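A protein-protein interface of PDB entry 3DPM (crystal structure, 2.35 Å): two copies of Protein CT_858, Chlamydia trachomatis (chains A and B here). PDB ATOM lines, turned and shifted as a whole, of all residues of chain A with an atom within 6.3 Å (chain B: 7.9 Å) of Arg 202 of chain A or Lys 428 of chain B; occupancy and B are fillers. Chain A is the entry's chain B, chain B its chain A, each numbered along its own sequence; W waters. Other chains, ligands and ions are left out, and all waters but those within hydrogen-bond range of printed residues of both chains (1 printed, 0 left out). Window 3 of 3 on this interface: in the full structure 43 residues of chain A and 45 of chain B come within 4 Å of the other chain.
Ala 198 of chain A touches none of the printed residues of chain B. Arg 202 of chain A touches just these residues of chain B: Lys 428 (2.5 Å), Gly 429 (3.9 Å), Asp 430 (3.1 Å) and Glu 432 (3.7 Å). No residue of chain B comes within 4 Å of Ala 203 of chain A. Printed residues of chain B within 4 Å of Pro 204 of chain A: Glu 432 and Leu 433. Gln 421 of chain B touches none of the printed residues of chain A. Of the printed residues of chain A, Trp 426 of chain B touches Ile 197 (3.1 Å). Lys 428 of chain B touches just these residues of chain A: Ser 200 (3.5 Å) and Arg 202 (2.5 Å). Printed residues of chain A within 4 Å of Asp 430 of chain B: Arg 202 (3.1 Å). Of the printed residues of chain A, Glu 432 of chain B touches Ile 201 (3.999 Å), Arg 202 (3.7 Å) and Pro 204 (3.998 Å). Of the printed residues of chain A, Leu 433 of chain B touches Pro 204 (3.9 Å) and Gln 205 (3.9 Å). The nearest residue of chain A that does not touch Lys 428 of chain B is Ile 197 of chain A (4.4 Å). The nearest printed residue of chain B that does not touch Pro 204 of chain A is Ser 434 of chain B (7.1 Å).
Of the 15 printed residues of chain B, 7 touch a printed residue of chain A. Hydrophobic or aromatic side chains of chain B within 4 Å of the printed part of chain A: Trp 426 and Leu 433. Hydrophobic or aromatic side chains of chain A that line the printed part of chain B: Ile 197, Ile 201 and Pro 204.
Water W1 bridges the backbone NH of Gln 205 of chain A (2.9 Å) and the backbone carbonyl oxygen of Leu 433 of chain B (3.1 Å).
The backbone carbonyl oxygen (O) of Ser 200 of chain A sits close to the backbone carbonyl oxygen (O) of Lys 428 of chain B (3.5 Å). The guanidinium group of Arg 202 of chain A sits at hydrogen-bond distance from the backbone carbonyl oxygen of Lys 428 of chain B (2.5 Å).
Ile 197 of chain A touches Ser 427 of chain B (CD1 to CA, 3.8 Å). Gly 429 of chain B touches Ile 197 of chain A (CA to CG2, 3.3 Å). Ile 201 of chain A touches Gly 429 of chain B. Glu 432 of chain B touches Ile 201 of chain A. N of Arg 202 of chain A touches O of Gly 429 of chain B, at 3.9 Å. Asp 430 of chain B touches Arg 202 of chain A (CB to NH2, 3.1 Å). Arg 202 of chain A touches Glu 432 of chain B. CD of Pro 204 of chain A touches CB of Glu 432 of chain B, 3.998 Å away. Pro 204 of chain A touches Leu 433 of chain B. Leu 433 of chain B touches Gln 205 of chain A.
No position is printed for both chains.
The backbone carbonyl oxygen of Leu 423 of chain B is in hydrogen-bond range of the side-chain hydroxyl of Ser 427 of chain B (3.4 Å). The side-chain carboxylate (OD2) of Asp 430 of chain B is in hydrogen-bond range of the backbone NH (N) of Thr 435 of chain B. O of Cys 425 of chain B lies within hydrogen-bond range of N of Asp 430 of chain B, 3.0 Å away. O of Asn 424 of chain B sits at hydrogen-bond distance from OG of Ser 427 of chain B. O of Ile 197 of chain A sits at hydrogen-bond distance from OG of Ser 200 of chain A, 2.8 Å away. NH1 of Arg 202 of chain A sits at hydrogen-bond distance from O of Ser 200 of chain A (3.2 Å).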
ATOM      1  N   ILE A 197     -11.595   9.064 -19.736  1.00  0.00           N
ATOM      2  CA  ILE A 197     -12.709   8.460 -19.035  1.00  0.00           C
ATOM      3  C   ILE A 197     -12.398   8.071 -17.589  1.00  0.00           C
ATOM      4  O   ILE A 197     -13.294   8.028 -16.753  1.00  0.00           O
ATOM      5  CB  ILE A 197     -13.164   7.248 -19.860  1.00  0.00           C
ATOM      6  CG1 ILE A 197     -13.657   7.757 -21.218  1.00  0.00           C
ATOM      7  CG2 ILE A 197     -14.211   6.445 -19.126  1.00  0.00           C
ATOM      8  CD1 ILE A 197     -13.821   6.680 -22.252  1.00  0.00           C
ATOM      9  N   ALA A 198     -11.123   7.819 -17.297  1.00  0.00           N
ATOM     10  CA  ALA A 198     -10.676   7.416 -15.964  1.00  0.00           C
ATOM     11  C   ALA A 198     -11.366   8.076 -14.763  1.00  0.00           C
ATOM     12  O   ALA A 198     -12.039   7.404 -13.991  1.00  0.00           O
ATOM     13  CB  ALA A 198      -9.159   7.592 -15.859  1.00  0.00           C
ATOM     14  N   SER A 200     -14.071   9.426 -14.294  1.00  0.00           N
ATOM     15  CA  SER A 200     -15.506   9.208 -14.189  1.00  0.00           C
ATOM     16  C   SER A 200     -15.920   7.746 -14.017  1.00  0.00           C
ATOM     17  O   SER A 200     -17.109   7.433 -14.050  1.00  0.00           O
ATOM     18  CB  SER A 200     -16.222   9.811 -15.402  1.00  0.00           C
ATOM     19  OG  SER A 200     -15.773   9.233 -16.615  1.00  0.00           O
ATOM     20  N   ILE A 201     -14.953   6.853 -13.821  1.00  0.00           N
ATOM     21  CA  ILE A 201     -15.246   5.428 -13.629  1.00  0.00           C
ATOM     22  C   ILE A 201     -15.818   5.144 -12.235  1.00  0.00           C
ATOM     23  O   ILE A 201     -15.221   5.513 -11.226  1.00  0.00           O
ATOM     24  CB  ILE A 201     -13.977   4.559 -13.804  1.00  0.00           C
ATOM     25  CG1 ILE A 201     -13.483   4.638 -15.248  1.00  0.00           C
ATOM     26  CG2 ILE A 201     -14.274   3.113 -13.416  1.00  0.00           C
ATOM     27  CD1 ILE A 201     -12.219   3.853 -15.506  1.00  0.00           C
ATOM     28  N   ARG A 202     -16.962   4.470 -12.176  1.00  0.00           N
ATOM     29  CA  ARG A 202     -17.588   4.153 -10.895  1.00  0.00           C
ATOM     30  C   ARG A 202     -17.518   2.678 -10.515  1.00  0.00           C
ATOM     31  O   ARG A 202     -17.697   1.797 -11.355  1.00  0.00           O
ATOM     32  CB  ARG A 202     -19.059   4.586 -10.896  1.00  0.00           C
ATOM     33  CG  ARG A 202     -19.839   4.206 -12.157  1.00  0.00           C
ATOM     34  CD  ARG A 202     -19.603   5.248 -13.246  1.00  0.00           C
ATOM     35  NE  ARG A 202     -20.532   5.130 -14.365  1.00  0.00           N
ATOM     36  CZ  ARG A 202     -20.766   6.103 -15.242  1.00  0.00           C
ATOM     37  NH1 ARG A 202     -20.136   7.266 -15.126  1.00  0.00           N
ATOM     38  NH2 ARG A 202     -21.631   5.914 -16.232  1.00  0.00           N
ATOM     39  N   ALA A 203     -17.269   2.421  -9.235  1.00  0.00           N
ATOM     40  CA  ALA A 203     -17.198   1.061  -8.717  1.00  0.00           C
ATOM     41  C   ALA A 203     -18.496   0.334  -9.053  1.00  0.00           C
ATOM     42  O   ALA A 203     -19.569   0.935  -9.069  1.00  0.00           O
ATOM     43  CB  ALA A 203     -16.983   1.085  -7.207  1.00  0.00           C
ATOM     44  N   PRO A 204     -18.419  -0.975  -9.320  1.00  0.00           N
ATOM     45  CA  PRO A 204     -19.626  -1.733  -9.654  1.00  0.00           C
ATOM     46  C   PRO A 204     -20.667  -1.766  -8.539  1.00  0.00           C
ATOM     47  O   PRO A 204     -20.350  -2.049  -7.381  1.00  0.00           O
ATOM     48  CB  PRO A 204     -19.078  -3.118  -9.994  1.00  0.00           C
ATOM     49  CG  PRO A 204     -17.883  -3.227  -9.101  1.00  0.00           C
ATOM     50  CD  PRO A 204     -17.246  -1.860  -9.239  1.00  0.00           C
ATOM     51  N   GLN A 205     -21.909  -1.464  -8.904  1.00  0.00           N
ATOM     52  CA  GLN A 205     -23.037  -1.466  -7.974  1.00  0.00           C
ATOM     53  C   GLN A 205     -24.066  -2.480  -8.453  1.00  0.00           C
ATOM     54  O   GLN A 205     -24.265  -2.633  -9.653  1.00  0.00           O
ATOM     55  CB  GLN A 205     -23.714  -0.094  -7.919  1.00  0.00           C
ATOM     56  CG  GLN A 205     -22.945   0.992  -7.201  1.00  0.00           C
ATOM     57  CD  GLN A 205     -23.872   1.921  -6.434  1.00  0.00           C
ATOM     58  OE1 GLN A 205     -24.864   2.416  -6.979  1.00  0.00           O
ATOM     59  NE2 GLN A 205     -23.557   2.161  -5.163  1.00  0.00           N
ATOM     60  N   GLN B 421     -25.115   2.003 -27.762  1.00  0.00           N
ATOM     61  CA  GLN B 421     -25.273   1.906 -26.312  1.00  0.00           C
ATOM     62  C   GLN B 421     -23.954   1.530 -25.643  1.00  0.00           C
ATOM     63  O   GLN B 421     -23.628   2.042 -24.570  1.00  0.00           O
ATOM     64  CB  GLN B 421     -26.357   0.879 -25.951  1.00  0.00           C
ATOM     65  CG  GLN B 421     -27.779   1.343 -26.277  1.00  0.00           C
ATOM     66  CD  GLN B 421     -28.852   0.293 -25.995  1.00  0.00           C
ATOM     67  OE1 GLN B 421     -29.081  -0.085 -24.845  1.00  0.00           O
ATOM     68  NE2 GLN B 421     -29.518  -0.178 -27.051  1.00  0.00           N
ATOM     69  N   VAL B 422     -23.190   0.645 -26.281  1.00  0.00           N
ATOM     70  CA  VAL B 422     -21.909   0.231 -25.732  1.00  0.00           C
ATOM     71  C   VAL B 422     -20.923   1.394 -25.771  1.00  0.00           C
ATOM     72  O   VAL B 422     -20.158   1.612 -24.824  1.00  0.00           O
ATOM     73  CB  VAL B 422     -21.313  -0.956 -26.519  1.00  0.00           C
ATOM     74  CG1 VAL B 422     -19.828  -1.111 -26.195  1.00  0.00           C
ATOM     75  CG2 VAL B 422     -22.054  -2.236 -26.161  1.00  0.00           C
ATOM     76  N   LEU B 423     -20.940   2.141 -26.869  1.00  0.00           N
ATOM     77  CA  LEU B 423     -20.042   3.279 -27.012  1.00  0.00           C
ATOM     78  C   LEU B 423     -20.383   4.345 -25.982  1.00  0.00           C
ATOM     79  O   LEU B 423     -19.496   4.959 -25.396  1.00  0.00           O
ATOM     80  CB  LEU B 423     -20.136   3.863 -28.423  1.00  0.00           C
ATOM     81  CG  LEU B 423     -19.727   2.921 -29.556  1.00  0.00           C
ATOM     82  CD1 LEU B 423     -19.789   3.683 -30.866  1.00  0.00           C
ATOM     83  CD2 LEU B 423     -18.327   2.383 -29.337  1.00  0.00           C
ATOM     84  N   ASN B 424     -21.671   4.556 -25.744  1.00  0.00           N
ATOM     85  CA  ASN B 424     -22.080   5.554 -24.767  1.00  0.00           C
ATOM     86  C   ASN B 424     -21.605   5.165 -23.374  1.00  0.00           C
ATOM     87  O   ASN B 424     -21.132   6.008 -22.620  1.00  0.00           O
ATOM     88  CB  ASN B 424     -23.598   5.721 -24.765  1.00  0.00           C
ATOM     89  CG  ASN B 424     -24.020   7.079 -24.244  1.00  0.00           C
ATOM     90  OD1 ASN B 424     -23.588   8.114 -24.761  1.00  0.00           O
ATOM     91  ND2 ASN B 424     -24.862   7.087 -23.217  1.00  0.00           N
ATOM     92  N   CYS B 425     -21.739   3.888 -23.028  1.00  0.00           N
ATOM     93  CA  CYS B 425     -21.283   3.409 -21.727  1.00  0.00           C
ATOM     94  C   CYS B 425     -19.783   3.621 -21.556  1.00  0.00           C
ATOM     95  O   CYS B 425     -19.325   4.067 -20.505  1.00  0.00           O
ATOM     96  CB  CYS B 425     -21.590   1.921 -21.560  1.00  0.00           C
ATOM     97  SG  CYS B 425     -23.282   1.578 -21.085  1.00  0.00           S
ATOM     98  N   TRP B 426     -19.023   3.292 -22.593  1.00  0.00           N
ATOM     99  CA  TRP B 426     -17.579   3.444 -22.559  1.00  0.00           C
ATOM    100  C   TRP B 426     -17.199   4.887 -22.274  1.00  0.00           C
ATOM    101  O   TRP B 426     -16.366   5.156 -21.403  1.00  0.00           O
ATOM    102  CB  TRP B 426     -16.970   3.001 -23.895  1.00  0.00           C
ATOM    103  CG  TRP B 426     -15.474   3.059 -23.928  1.00  0.00           C
ATOM    104  CD1 TRP B 426     -14.703   4.006 -24.541  1.00  0.00           C
ATOM    105  CD2 TRP B 426     -14.568   2.143 -23.298  1.00  0.00           C
ATOM    106  NE1 TRP B 426     -13.369   3.736 -24.329  1.00  0.00           N
ATOM    107  CE2 TRP B 426     -13.258   2.599 -23.571  1.00  0.00           C
ATOM    108  CE3 TRP B 426     -14.735   0.985 -22.528  1.00  0.00           C
ATOM    109  CZ2 TRP B 426     -12.114   1.932 -23.099  1.00  0.00           C
ATOM    110  CZ3 TRP B 426     -13.601   0.320 -22.058  1.00  0.00           C
ATOM    111  CH2 TRP B 426     -12.304   0.800 -22.347  1.00  0.00           C
ATOM    112  N   SER B 427     -17.821   5.808 -23.003  1.00  0.00           N
ATOM    113  CA  SER B 427     -17.539   7.230 -22.842  1.00  0.00           C
ATOM    114  C   SER B 427     -17.928   7.779 -21.464  1.00  0.00           C
ATOM    115  O   SER B 427     -17.403   8.809 -21.042  1.00  0.00           O
ATOM    116  CB  SER B 427     -18.254   8.025 -23.934  1.00  0.00           C
ATOM    117  OG  SER B 427     -19.661   7.909 -23.803  1.00  0.00           O
ATOM    118  N   LYS B 428     -18.836   7.097 -20.765  1.00  0.00           N
ATOM    119  CA  LYS B 428     -19.265   7.540 -19.435  1.00  0.00           C
ATOM    120  C   LYS B 428     -18.487   6.871 -18.307  1.00  0.00           C
ATOM    121  O   LYS B 428     -18.665   7.218 -17.143  1.00  0.00           O
ATOM    122  CB  LYS B 428     -20.742   7.230 -19.194  1.00  0.00           C
ATOM    123  CG  LYS B 428     -21.744   7.944 -20.080  1.00  0.00           C
ATOM    124  CD  LYS B 428     -23.145   7.494 -19.652  1.00  0.00           C
ATOM    125  CE  LYS B 428     -24.250   8.281 -20.333  1.00  0.00           C
ATOM    126  NZ  LYS B 428     -25.587   7.985 -19.720  1.00  0.00           N
ATOM    127  N   GLY B 429     -17.647   5.899 -18.644  1.00  0.00           N
ATOM    128  CA  GLY B 429     -16.896   5.197 -17.619  1.00  0.00           C
ATOM    129  C   GLY B 429     -17.713   4.099 -16.957  1.00  0.00           C
ATOM    130  O   GLY B 429     -17.301   3.530 -15.939  1.00  0.00           O
ATOM    131  N   ASP B 430     -18.877   3.807 -17.528  1.00  0.00           N
ATOM    132  CA  ASP B 430     -19.761   2.768 -16.995  1.00  0.00           C
ATOM    133  C   ASP B 430     -19.297   1.461 -17.615  1.00  0.00           C
ATOM    134  O   ASP B 430     -20.007   0.833 -18.397  1.00  0.00           O
ATOM    135  CB  ASP B 430     -21.212   3.073 -17.387  1.00  0.00           C
ATOM    136  CG  ASP B 430     -22.206   2.087 -16.793  1.00  0.00           C
ATOM    137  OD1 ASP B 430     -21.911   1.511 -15.719  1.00  0.00           O
ATOM    138  OD2 ASP B 430     -23.294   1.903 -17.392  1.00  0.00           O
ATOM    139  N   ILE B 431     -18.093   1.053 -17.243  1.00  0.00           N
ATOM    140  CA  ILE B 431     -17.493  -0.132 -17.813  1.00  0.00           C
ATOM    141  C   ILE B 431     -17.171  -1.264 -16.851  1.00  0.00           C
ATOM    142  O   ILE B 431     -16.744  -2.335 -17.275  1.00  0.00           O
ATOM    143  CB  ILE B 431     -16.229   0.277 -18.551  1.00  0.00           C
ATOM    144  CG1 ILE B 431     -15.195   0.803 -17.545  1.00  0.00           C
ATOM    145  CG2 ILE B 431     -16.572   1.383 -19.554  1.00  0.00           C
ATOM    146  CD1 ILE B 431     -13.869   1.253 -18.196  1.00  0.00           C
ATOM    147  N   GLU B 432     -17.362  -1.032 -15.557  1.00  0.00           N
ATOM    148  CA  GLU B 432     -17.102  -2.070 -14.571  1.00  0.00           C
ATOM    149  C   GLU B 432     -18.301  -3.010 -14.548  1.00  0.00           C
ATOM    150  O   GLU B 432     -18.150  -4.227 -14.489  1.00  0.00           O
ATOM    151  CB  GLU B 432     -16.857  -1.444 -13.196  1.00  0.00           C
ATOM    152  CG  GLU B 432     -15.545  -0.666 -13.111  1.00  0.00           C
ATOM    153  CD  GLU B 432     -14.324  -1.537 -13.401  1.00  0.00           C
ATOM    154  OE1 GLU B 432     -13.204  -0.991 -13.536  1.00  0.00           O
ATOM    155  OE2 GLU B 432     -14.482  -2.774 -13.490  1.00  0.00           O
ATOM    156  N   LEU B 433     -19.493  -2.434 -14.598  1.00  0.00           N
ATOM    157  CA  LEU B 433     -20.732  -3.205 -14.634  1.00  0.00           C
ATOM    158  C   LEU B 433     -21.775  -2.253 -15.213  1.00  0.00           C
ATOM    159  O   LEU B 433     -22.557  -1.634 -14.498  1.00  0.00           O
ATOM    160  CB  LEU B 433     -21.119  -3.675 -13.235  1.00  0.00           C
ATOM    161  CG  LEU B 433     -22.164  -4.793 -13.109  1.00  0.00           C
ATOM    162  CD1 LEU B 433     -21.793  -5.975 -13.976  1.00  0.00           C
ATOM    163  CD2 LEU B 433     -22.244  -5.228 -11.658  1.00  0.00           C
ATOM    164  N   SER B 434     -21.749  -2.133 -16.533  1.00  0.00           N
ATOM    165  CA  SER B 434     -22.637  -1.237 -17.255  1.00  0.00           C
ATOM    166  C   SER B 434     -24.117  -1.354 -16.910  1.00  0.00           C
ATOM    167  O   SER B 434     -24.576  -2.357 -16.374  1.00  0.00           O
ATOM    168  CB  SER B 434     -22.483  -1.470 -18.752  1.00  0.00           C
ATOM    169  OG  SER B 434     -23.117  -2.690 -19.107  1.00  0.00           O
ATOM    170  N   THR B 435     -24.856  -0.305 -17.243  1.00  0.00           N
ATOM    171  CA  THR B 435     -26.295  -0.278 -17.053  1.00  0.00           C
ATOM    172  C   THR B 435     -26.789  -1.431 -17.923  1.00  0.00           C
ATOM    173  O   THR B 435     -26.096  -1.847 -18.844  1.00  0.00           O
ATOM    174  CB  THR B 435     -26.881   1.042 -17.582  1.00  0.00           C
ATOM    175  OG1 THR B 435     -28.306   1.012 -17.480  1.00  0.00           O
ATOM    176  CG2 THR B 435     -26.505   1.246 -19.035  1.00  0.00           C
HETATM  177  O   HOH W   1     -21.905  -0.548 -11.698  1.00  0.00           O
